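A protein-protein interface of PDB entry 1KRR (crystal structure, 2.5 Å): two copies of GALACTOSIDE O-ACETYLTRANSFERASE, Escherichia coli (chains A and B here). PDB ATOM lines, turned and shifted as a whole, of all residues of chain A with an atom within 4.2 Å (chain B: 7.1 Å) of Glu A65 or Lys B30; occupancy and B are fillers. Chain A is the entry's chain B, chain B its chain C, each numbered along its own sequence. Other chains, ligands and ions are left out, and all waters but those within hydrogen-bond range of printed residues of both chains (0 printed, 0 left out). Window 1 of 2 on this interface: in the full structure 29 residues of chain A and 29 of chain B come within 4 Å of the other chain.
Of the printed residues of chain B, Pro A41 touches Leu B27, Lys B30, Thr B31 and Tyr B34. Of chain B, only Lys B30 comes within 4 Å of Glu A65. Tyr A83 touches none of the printed residues of chain B. Of the printed residues of chain B, Phe A86 touches Met B33, Tyr B69 and Phe B70. Of the printed residues of chain A, Leu B27 touches Pro A41. Printed residues of chain A within 4 Å of Met B33: Phe A86 (3.7 Å). Of the printed residues of chain A, Phe B70 touches Phe A86. Ser B71 touches none of the printed residues of chain A. The nearest residue of chain B that does not touch Glu A65 is Met B33 (5.4 Å). The nearest printed residue of chain B that does not touch Pro A67 is Met B33 (6.1 Å).
Among the printed residues, pairs that only touch across the chains: Pro A41 with Lys B30 (3.2 Å), Phe A86 with Phe B70 (3.2 Å), Pro A67 with Tyr B69 (3.5 Å), Pro A41 with Tyr B34 (3.6 Å), Pro A41 with Leu B27 (3.6 Å), Phe A86 with Tyr B69 (3.6 Å), Phe A86 with Met B33 (3.7 Å) and Pro A41 with Thr B31 (3.8 Å).
No position is printed for both chains. Of the 9 pairs that touch across the chains among the printed residues, none has its exchanged pair printed and touching as well.
The side-chain carboxylate of Glu A65 lies within hydrogen-bond range of the indole nitrogen of Trp A63, at 3.1 Å. N of Glu A65 is in hydrogen-bond range of O of Ala A84 (3.0 Å). The backbone carbonyl oxygen (O) of Leu B27 sits at hydrogen-bond distance from the side-chain hydroxyl (OG1) of Thr B31.
Of the 18 printed residues of chain B, 7 touch a printed residue of chain A. Of the 10 printed residues of chain A, 4 touch a printed residue of chain B. Among the printed residues, 9 pairs touch across the chains.
OE2 of Glu A65 is in salt-bridge range of NZ of Lys B30 (3.3 Å).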
ATOM      1  N   PRO A  41      25.022 -19.302 -13.138  1.00  0.00           N
ATOM      2  CA  PRO A  41      24.077 -20.040 -13.995  1.00  0.00           C
ATOM      3  C   PRO A  41      23.353 -19.180 -15.004  1.00  0.00           C
ATOM      4  O   PRO A  41      22.913 -19.662 -16.037  1.00  0.00           O
ATOM      5  CB  PRO A  41      23.106 -20.691 -13.008  1.00  0.00           C
ATOM      6  CG  PRO A  41      23.364 -20.016 -11.679  1.00  0.00           C
ATOM      7  CD  PRO A  41      24.801 -19.601 -11.713  1.00  0.00           C
ATOM      8  N   TRP A  63      25.756 -29.379 -24.073  1.00  0.00           N
ATOM      9  CA  TRP A  63      25.528 -28.805 -22.775  1.00  0.00           C
ATOM     10  C   TRP A  63      26.374 -29.513 -21.741  1.00  0.00           C
ATOM     11  O   TRP A  63      26.572 -30.723 -21.802  1.00  0.00           O
ATOM     12  CB  TRP A  63      24.062 -28.884 -22.387  1.00  0.00           C
ATOM     13  CG  TRP A  63      23.792 -28.159 -21.103  1.00  0.00           C
ATOM     14  CD1 TRP A  63      22.985 -28.569 -20.081  1.00  0.00           C
ATOM     15  CD2 TRP A  63      24.371 -26.915 -20.686  1.00  0.00           C
ATOM     16  NE1 TRP A  63      23.027 -27.659 -19.052  1.00  0.00           N
ATOM     17  CE2 TRP A  63      23.872 -26.634 -19.397  1.00  0.00           C
ATOM     18  CE3 TRP A  63      25.267 -26.009 -21.279  1.00  0.00           C
ATOM     19  CZ2 TRP A  63      24.240 -25.476 -18.680  1.00  0.00           C
ATOM     20  CZ3 TRP A  63      25.632 -24.863 -20.571  1.00  0.00           C
ATOM     21  CH2 TRP A  63      25.116 -24.608 -19.281  1.00  0.00           C
ATOM     22  N   VAL A  64      26.897 -28.748 -20.797  1.00  0.00           N
ATOM     23  CA  VAL A  64      27.720 -29.308 -19.754  1.00  0.00           C
ATOM     24  C   VAL A  64      27.397 -28.585 -18.472  1.00  0.00           C
ATOM     25  O   VAL A  64      27.533 -27.368 -18.368  1.00  0.00           O
ATOM     26  CB  VAL A  64      29.230 -29.168 -20.071  1.00  0.00           C
ATOM     27  CG1 VAL A  64      30.067 -29.916 -19.018  1.00  0.00           C
ATOM     28  CG2 VAL A  64      29.514 -29.728 -21.461  1.00  0.00           C
ATOM     29  N   GLU A  65      26.943 -29.354 -17.493  1.00  0.00           N
ATOM     30  CA  GLU A  65      26.598 -28.801 -16.208  1.00  0.00           C
ATOM     31  C   GLU A  65      27.867 -28.577 -15.392  1.00  0.00           C
ATOM     32  O   GLU A  65      28.549 -29.522 -15.019  1.00  0.00           O
ATOM     33  CB  GLU A  65      25.667 -29.760 -15.465  1.00  0.00           C
ATOM     34  CG  GLU A  65      24.192 -29.448 -15.599  1.00  0.00           C
ATOM     35  CD  GLU A  65      23.870 -28.002 -15.273  1.00  0.00           C
ATOM     36  OE1 GLU A  65      24.427 -27.447 -14.296  1.00  0.00           O
ATOM     37  OE2 GLU A  65      23.052 -27.419 -16.008  1.00  0.00           O
ATOM     38  N   PRO A  66      28.225 -27.313 -15.139  1.00  0.00           N
ATOM     39  CA  PRO A  66      29.437 -27.131 -14.342  1.00  0.00           C
ATOM     40  C   PRO A  66      29.203 -27.707 -12.941  1.00  0.00           C
ATOM     41  O   PRO A  66      28.077 -27.741 -12.451  1.00  0.00           O
ATOM     42  CB  PRO A  66      29.640 -25.615 -14.327  1.00  0.00           C
ATOM     43  CG  PRO A  66      28.310 -25.040 -14.686  1.00  0.00           C
ATOM     44  CD  PRO A  66      27.625 -26.035 -15.554  1.00  0.00           C
ATOM     45  N   PRO A  67      30.266 -28.151 -12.270  1.00  0.00           N
ATOM     46  CA  PRO A  67      31.651 -28.147 -12.725  1.00  0.00           C
ATOM     47  C   PRO A  67      32.065 -29.292 -13.627  1.00  0.00           C
ATOM     48  O   PRO A  67      31.464 -30.355 -13.629  1.00  0.00           O
ATOM     49  CB  PRO A  67      32.444 -28.136 -11.428  1.00  0.00           C
ATOM     50  CG  PRO A  67      31.578 -28.834 -10.458  1.00  0.00           C
ATOM     51  CD  PRO A  67      30.145 -28.686 -10.907  1.00  0.00           C
ATOM     52  N   TYR A  83      25.289 -34.058 -23.852  1.00  0.00           N
ATOM     53  CA  TYR A  83      24.846 -33.619 -22.539  1.00  0.00           C
ATOM     54  C   TYR A  83      25.685 -34.319 -21.481  1.00  0.00           C
ATOM     55  O   TYR A  83      25.836 -35.544 -21.486  1.00  0.00           O
ATOM     56  CB  TYR A  83      23.370 -33.928 -22.307  1.00  0.00           C
ATOM     57  CG  TYR A  83      22.908 -33.488 -20.950  1.00  0.00           C
ATOM     58  CD1 TYR A  83      22.493 -32.190 -20.730  1.00  0.00           C
ATOM     59  CD2 TYR A  83      22.930 -34.350 -19.876  1.00  0.00           C
ATOM     60  CE1 TYR A  83      22.112 -31.753 -19.467  1.00  0.00           C
ATOM     61  CE2 TYR A  83      22.553 -33.927 -18.604  1.00  0.00           C
ATOM     62  CZ  TYR A  83      22.145 -32.620 -18.403  1.00  0.00           C
ATOM     63  OH  TYR A  83      21.792 -32.176 -17.139  1.00  0.00           O
ATOM     64  N   ALA A  84      26.244 -33.527 -20.584  1.00  0.00           N
ATOM     65  CA  ALA A  84      27.067 -34.053 -19.521  1.00  0.00           C
ATOM     66  C   ALA A  84      26.569 -33.388 -18.275  1.00  0.00           C
ATOM     67  O   ALA A  84      26.436 -32.174 -18.227  1.00  0.00           O
ATOM     68  CB  ALA A  84      28.538 -33.703 -19.750  1.00  0.00           C
ATOM     69  N   ASN A  85      26.287 -34.194 -17.265  1.00  0.00           N
ATOM     70  CA  ASN A  85      25.796 -33.678 -16.010  1.00  0.00           C
ATOM     71  C   ASN A  85      26.974 -33.395 -15.073  1.00  0.00           C
ATOM     72  O   ASN A  85      28.107 -33.727 -15.391  1.00  0.00           O
ATOM     73  CB  ASN A  85      24.826 -34.686 -15.399  1.00  0.00           C
ATOM     74  CG  ASN A  85      23.674 -34.023 -14.722  1.00  0.00           C
ATOM     75  OD1 ASN A  85      23.838 -32.979 -14.121  1.00  0.00           O
ATOM     76  ND2 ASN A  85      22.496 -34.614 -14.818  1.00  0.00           N
ATOM     77  N   PHE A  86      26.690 -32.780 -13.930  1.00  0.00           N
ATOM     78  CA  PHE A  86      27.685 -32.415 -12.931  1.00  0.00           C
ATOM     79  C   PHE A  86      28.904 -33.309 -12.813  1.00  0.00           C
ATOM     80  O   PHE A  86      28.818 -34.528 -12.930  1.00  0.00           O
ATOM     81  CB  PHE A  86      27.066 -32.354 -11.531  1.00  0.00           C
ATOM     82  CG  PHE A  86      25.815 -31.537 -11.426  1.00  0.00           C
ATOM     83  CD1 PHE A  86      25.838 -30.179 -11.639  1.00  0.00           C
ATOM     84  CD2 PHE A  86      24.628 -32.122 -11.016  1.00  0.00           C
ATOM     85  CE1 PHE A  86      24.696 -29.411 -11.435  1.00  0.00           C
ATOM     86  CE2 PHE A  86      23.493 -31.361 -10.813  1.00  0.00           C
ATOM     87  CZ  PHE A  86      23.531 -30.004 -11.022  1.00  0.00           C
ATOM     88  N   PRO B  23      12.656 -25.153 -17.699  1.00  0.00           N
ATOM     89  CA  PRO B  23      13.984 -24.527 -17.725  1.00  0.00           C
ATOM     90  C   PRO B  23      14.121 -23.362 -16.734  1.00  0.00           C
ATOM     91  O   PRO B  23      15.141 -23.227 -16.040  1.00  0.00           O
ATOM     92  CB  PRO B  23      14.144 -24.063 -19.180  1.00  0.00           C
ATOM     93  CG  PRO B  23      13.168 -24.867 -19.960  1.00  0.00           C
ATOM     94  CD  PRO B  23      12.015 -25.139 -19.025  1.00  0.00           C
ATOM     95  N   LYS B  25      12.406 -22.895 -14.043  1.00  0.00           N
ATOM     96  CA  LYS B  25      12.313 -23.466 -12.701  1.00  0.00           C
ATOM     97  C   LYS B  25      13.707 -23.931 -12.288  1.00  0.00           C
ATOM     98  O   LYS B  25      14.124 -23.757 -11.143  1.00  0.00           O
ATOM     99  CB  LYS B  25      11.337 -24.648 -12.712  1.00  0.00           C
ATOM    100  CG  LYS B  25      10.270 -24.612 -11.627  1.00  0.00           C
ATOM    101  CD  LYS B  25       9.599 -25.979 -11.492  1.00  0.00           C
ATOM    102  CE  LYS B  25       8.343 -25.888 -10.638  1.00  0.00           C
ATOM    103  NZ  LYS B  25       8.609 -25.279  -9.294  1.00  0.00           N
ATOM    104  N   ARG B  26      14.412 -24.524 -13.245  1.00  0.00           N
ATOM    105  CA  ARG B  26      15.767 -25.017 -13.046  1.00  0.00           C
ATOM    106  C   ARG B  26      16.727 -23.861 -12.767  1.00  0.00           C
ATOM    107  O   ARG B  26      17.592 -23.968 -11.894  1.00  0.00           O
ATOM    108  CB  ARG B  26      16.233 -25.771 -14.288  1.00  0.00           C
ATOM    109  CG  ARG B  26      16.438 -27.269 -14.094  1.00  0.00           C
ATOM    110  CD  ARG B  26      16.547 -27.960 -15.427  1.00  0.00           C
ATOM    111  NE  ARG B  26      15.217 -28.159 -15.975  1.00  0.00           N
ATOM    112  CZ  ARG B  26      14.913 -28.160 -17.268  1.00  0.00           C
ATOM    113  NH1 ARG B  26      15.851 -27.967 -18.198  1.00  0.00           N
ATOM    114  NH2 ARG B  26      13.659 -28.367 -17.629  1.00  0.00           N
ATOM    115  N   LEU B  27      16.579 -22.755 -13.495  1.00  0.00           N
ATOM    116  CA  LEU B  27      17.457 -21.606 -13.298  1.00  0.00           C
ATOM    117  C   LEU B  27      17.374 -20.991 -11.901  1.00  0.00           C
ATOM    118  O   LEU B  27      18.372 -20.520 -11.370  1.00  0.00           O
ATOM    119  CB  LEU B  27      17.169 -20.540 -14.339  1.00  0.00           C
ATOM    120  CG  LEU B  27      18.226 -19.434 -14.376  1.00  0.00           C
ATOM    121  CD1 LEU B  27      19.554 -20.026 -14.763  1.00  0.00           C
ATOM    122  CD2 LEU B  27      17.812 -18.349 -15.365  1.00  0.00           C
ATOM    123  N   ARG B  28      16.190 -20.974 -11.306  1.00  0.00           N
ATOM    124  CA  ARG B  28      16.060 -20.422  -9.962  1.00  0.00           C
ATOM    125  C   ARG B  28      16.811 -21.358  -9.043  1.00  0.00           C
ATOM    126  O   ARG B  28      17.530 -20.922  -8.152  1.00  0.00           O
ATOM    127  CB  ARG B  28      14.593 -20.357  -9.526  1.00  0.00           C
ATOM    128  CG  ARG B  28      13.667 -19.930 -10.641  1.00  0.00           C
ATOM    129  CD  ARG B  28      12.217 -20.351 -10.395  1.00  0.00           C
ATOM    130  NE  ARG B  28      11.347 -20.009 -11.526  1.00  0.00           N
ATOM    131  CZ  ARG B  28      10.071 -20.380 -11.618  1.00  0.00           C
ATOM    132  NH1 ARG B  28       9.546 -21.100 -10.635  1.00  0.00           N
ATOM    133  NH2 ARG B  28       9.323 -20.044 -12.678  1.00  0.00           N
ATOM    134  N   GLY B  29      16.642 -22.655  -9.279  1.00  0.00           N
ATOM    135  CA  GLY B  29      17.317 -23.648  -8.462  1.00  0.00           C
ATOM    136  C   GLY B  29      18.822 -23.495  -8.517  1.00  0.00           C
ATOM    137  O   GLY B  29      19.449 -23.202  -7.497  1.00  0.00           O
ATOM    138  N   LYS B  30      19.386 -23.696  -9.710  1.00  0.00           N
ATOM    139  CA  LYS B  30      20.824 -23.566  -9.936  1.00  0.00           C
ATOM    140  C   LYS B  30      21.363 -22.197  -9.510  1.00  0.00           C
ATOM    141  O   LYS B  30      22.571 -22.034  -9.359  1.00  0.00           O
ATOM    142  CB  LYS B  30      21.142 -23.802 -11.406  1.00  0.00           C
ATOM    143  CG  LYS B  30      20.328 -24.924 -12.019  1.00  0.00           C
ATOM    144  CD  LYS B  30      21.050 -26.256 -11.993  1.00  0.00           C
ATOM    145  CE  LYS B  30      20.512 -27.176 -13.092  1.00  0.00           C
ATOM    146  NZ  LYS B  30      20.343 -26.476 -14.424  1.00  0.00           N
ATOM    147  N   THR B  31      20.466 -21.228  -9.317  1.00  0.00           N
ATOM    148  CA  THR B  31      20.846 -19.886  -8.896  1.00  0.00           C
ATOM    149  C   THR B  31      21.059 -19.905  -7.398  1.00  0.00           C
ATOM    150  O   THR B  31      22.083 -19.426  -6.919  1.00  0.00           O
ATOM    151  CB  THR B  31      19.761 -18.842  -9.238  1.00  0.00           C
ATOM    152  OG1 THR B  31      19.786 -18.579 -10.636  1.00  0.00           O
ATOM    153  CG2 THR B  31      20.001 -17.531  -8.494  1.00  0.00           C
ATOM    154  N   LEU B  32      20.095 -20.434  -6.651  1.00  0.00           N
ATOM    155  CA  LEU B  32      20.241 -20.520  -5.199  1.00  0.00           C
ATOM    156  C   LEU B  32      21.384 -21.483  -4.887  1.00  0.00           C
ATOM    157  O   LEU B  32      22.114 -21.313  -3.917  1.00  0.00           O
ATOM    158  CB  LEU B  32      18.962 -21.040  -4.551  1.00  0.00           C
ATOM    159  CG  LEU B  32      17.797 -20.063  -4.503  1.00  0.00           C
ATOM    160  CD1 LEU B  32      16.519 -20.844  -4.242  1.00  0.00           C
ATOM    161  CD2 LEU B  32      18.040 -19.017  -3.417  1.00  0.00           C
ATOM    162  N   MET B  33      21.511 -22.505  -5.721  1.00  0.00           N
ATOM    163  CA  MET B  33      22.554 -23.494  -5.581  1.00  0.00           C
ATOM    164  C   MET B  33      23.910 -22.789  -5.705  1.00  0.00           C
ATOM    165  O   MET B  33      24.778 -22.955  -4.858  1.00  0.00           O
ATOM    166  CB  MET B  33      22.388 -24.557  -6.663  1.00  0.00           C
ATOM    167  CG  MET B  33      23.538 -25.527  -6.778  1.00  0.00           C
ATOM    168  SD  MET B  33      23.176 -26.671  -8.075  1.00  0.00           S
ATOM    169  CE  MET B  33      24.661 -26.677  -8.983  1.00  0.00           C
ATOM    170  N   TYR B  34      24.084 -21.989  -6.754  1.00  0.00           N
ATOM    171  CA  TYR B  34      25.328 -21.246  -6.958  1.00  0.00           C
ATOM    172  C   TYR B  34      25.631 -20.367  -5.729  1.00  0.00           C
ATOM    173  O   TYR B  34      26.759 -20.322  -5.239  1.00  0.00           O
ATOM    174  CB  TYR B  34      25.228 -20.391  -8.228  1.00  0.00           C
ATOM    175  CG  TYR B  34      26.416 -19.489  -8.471  1.00  0.00           C
ATOM    176  CD1 TYR B  34      26.461 -18.207  -7.922  1.00  0.00           C
ATOM    177  CD2 TYR B  34      27.515 -19.923  -9.226  1.00  0.00           C
ATOM    178  CE1 TYR B  34      27.571 -17.378  -8.112  1.00  0.00           C
ATOM    179  CE2 TYR B  34      28.638 -19.095  -9.421  1.00  0.00           C
ATOM    180  CZ  TYR B  34      28.654 -17.824  -8.860  1.00  0.00           C
ATOM    181  OH  TYR B  34      29.741 -16.996  -9.044  1.00  0.00           O
ATOM    182  N   GLU B  35      24.617 -19.681  -5.226  1.00  0.00           N
ATOM    183  CA  GLU B  35      24.789 -18.835  -4.068  1.00  0.00           C
ATOM    184  C   GLU B  35      25.238 -19.659  -2.846  1.00  0.00           C
ATOM    185  O   GLU B  35      25.995 -19.183  -1.995  1.00  0.00           O
ATOM    186  CB  GLU B  35      23.468 -18.127  -3.760  1.00  0.00           C
ATOM    187  CG  GLU B  35      23.329 -16.690  -4.262  1.00  0.00           C
ATOM    188  CD  GLU B  35      22.062 -16.028  -3.722  1.00  0.00           C
ATOM    189  OE1 GLU B  35      21.961 -15.840  -2.479  1.00  0.00           O
ATOM    190  OE2 GLU B  35      21.159 -15.701  -4.533  1.00  0.00           O
ATOM    191  N   PHE B  36      24.779 -20.898  -2.752  1.00  0.00           N
ATOM    192  CA  PHE B  36      25.138 -21.736  -1.613  1.00  0.00           C
ATOM    193  C   PHE B  36      26.547 -22.280  -1.787  1.00  0.00           C
ATOM    194  O   PHE B  36      27.405 -22.143  -0.917  1.00  0.00           O
ATOM    195  CB  PHE B  36      24.138 -22.901  -1.480  1.00  0.00           C
ATOM    196  CG  PHE B  36      24.333 -23.745  -0.246  1.00  0.00           C
ATOM    197  CD1 PHE B  36      23.902 -23.295   0.999  1.00  0.00           C
ATOM    198  CD2 PHE B  36      24.967 -24.976  -0.325  1.00  0.00           C
ATOM    199  CE1 PHE B  36      24.108 -24.060   2.154  1.00  0.00           C
ATOM    200  CE2 PHE B  36      25.179 -25.752   0.825  1.00  0.00           C
ATOM    201  CZ  PHE B  36      24.749 -25.289   2.067  1.00  0.00           C
ATOM    202  N   TYR B  69      24.753 -30.471  -5.289  1.00  0.00           N
ATOM    203  CA  TYR B  69      24.235 -30.344  -6.638  1.00  0.00           C
ATOM    204  C   TYR B  69      22.831 -30.948  -6.802  1.00  0.00           C
ATOM    205  O   TYR B  69      22.509 -31.987  -6.214  1.00  0.00           O
ATOM    206  CB  TYR B  69      25.212 -30.991  -7.613  1.00  0.00           C
ATOM    207  CG  TYR B  69      26.598 -30.389  -7.529  1.00  0.00           C
ATOM    208  CD1 TYR B  69      26.910 -29.200  -8.194  1.00  0.00           C
ATOM    209  CD2 TYR B  69      27.586 -30.983  -6.749  1.00  0.00           C
ATOM    210  CE1 TYR B  69      28.165 -28.622  -8.079  1.00  0.00           C
ATOM    211  CE2 TYR B  69      28.845 -30.416  -6.626  1.00  0.00           C
ATOM    212  CZ  TYR B  69      29.139 -29.235  -7.290  1.00  0.00           C
ATOM    213  OH  TYR B  69      30.404 -28.685  -7.164  1.00  0.00           O
ATOM    214  N   PHE B  70      21.991 -30.261  -7.577  1.00  0.00           N
ATOM    215  CA  PHE B  70      20.639 -30.720  -7.870  1.00  0.00           C
ATOM    216  C   PHE B  70      20.143 -30.069  -9.153  1.00  0.00           C
ATOM    217  O   PHE B  70      20.757 -29.135  -9.654  1.00  0.00           O
ATOM    218  CB  PHE B  70      19.667 -30.430  -6.707  1.00  0.00           C
ATOM    219  CG  PHE B  70      19.722 -29.020  -6.181  1.00  0.00           C
ATOM    220  CD1 PHE B  70      19.155 -27.973  -6.890  1.00  0.00           C
ATOM    221  CD2 PHE B  70      20.311 -28.748  -4.959  1.00  0.00           C
ATOM    222  CE1 PHE B  70      19.175 -26.677  -6.385  1.00  0.00           C
ATOM    223  CE2 PHE B  70      20.332 -27.442  -4.447  1.00  0.00           C
ATOM    224  CZ  PHE B  70      19.766 -26.413  -5.160  1.00  0.00           C
ATOM    225  N   SER B  71      19.040 -30.579  -9.686  1.00  0.00           N
ATOM    226  CA  SER B  71      18.465 -30.064 -10.914  1.00  0.00           C
ATOM    227  C   SER B  71      17.487 -28.934 -10.665  1.00  0.00           C
ATOM    228  O   SER B  71      17.571 -27.899 -11.308  1.00  0.00           O
ATOM    229  CB  SER B  71      17.765 -31.188 -11.669  1.00  0.00           C
ATOM    230  OG  SER B  71      18.617 -32.315 -11.771  1.00  0.00           O
ATOM    231  N   TYR B  72      16.557 -29.130  -9.736  1.00  0.00           N
ATOM    232  CA  TYR B  72      15.562 -28.108  -9.419  1.00  0.00           C
ATOM    233  C   TYR B  72      15.682 -27.657  -7.983  1.00  0.00           C
ATOM    234  O   TYR B  72      15.601 -26.472  -7.693  1.00  0.00           O
ATOM    235  CB  TYR B  72      14.152 -28.640  -9.635  1.00  0.00           C
ATOM    236  CG  TYR B  72      13.820 -28.910 -11.069  1.00  0.00           C
ATOM    237  CD1 TYR B  72      14.220 -30.087 -11.684  1.00  0.00           C
ATOM    238  CD2 TYR B  72      13.092 -27.992 -11.813  1.00  0.00           C
ATOM    239  CE1 TYR B  72      13.903 -30.347 -13.007  1.00  0.00           C
ATOM    240  CE2 TYR B  72      12.766 -28.239 -13.140  1.00  0.00           C
ATOM    241  CZ  TYR B  72      13.171 -29.418 -13.734  1.00  0.00           C
ATOM    242  OH  TYR B  72      12.831 -29.672 -15.053  1.00  0.00           O
ATOM    243  N   GLY B  73      15.874 -28.624  -7.088  1.00  0.00           N
ATOM    244  CA  GLY B  73      15.978 -28.348  -5.669  1.00  0.00           C
ATOM    245  C   GLY B  73      14.608 -28.364  -5.001  1.00  0.00           C
ATOM    246  O   GLY B  73      14.410 -28.944  -3.928  1.00  0.00           O
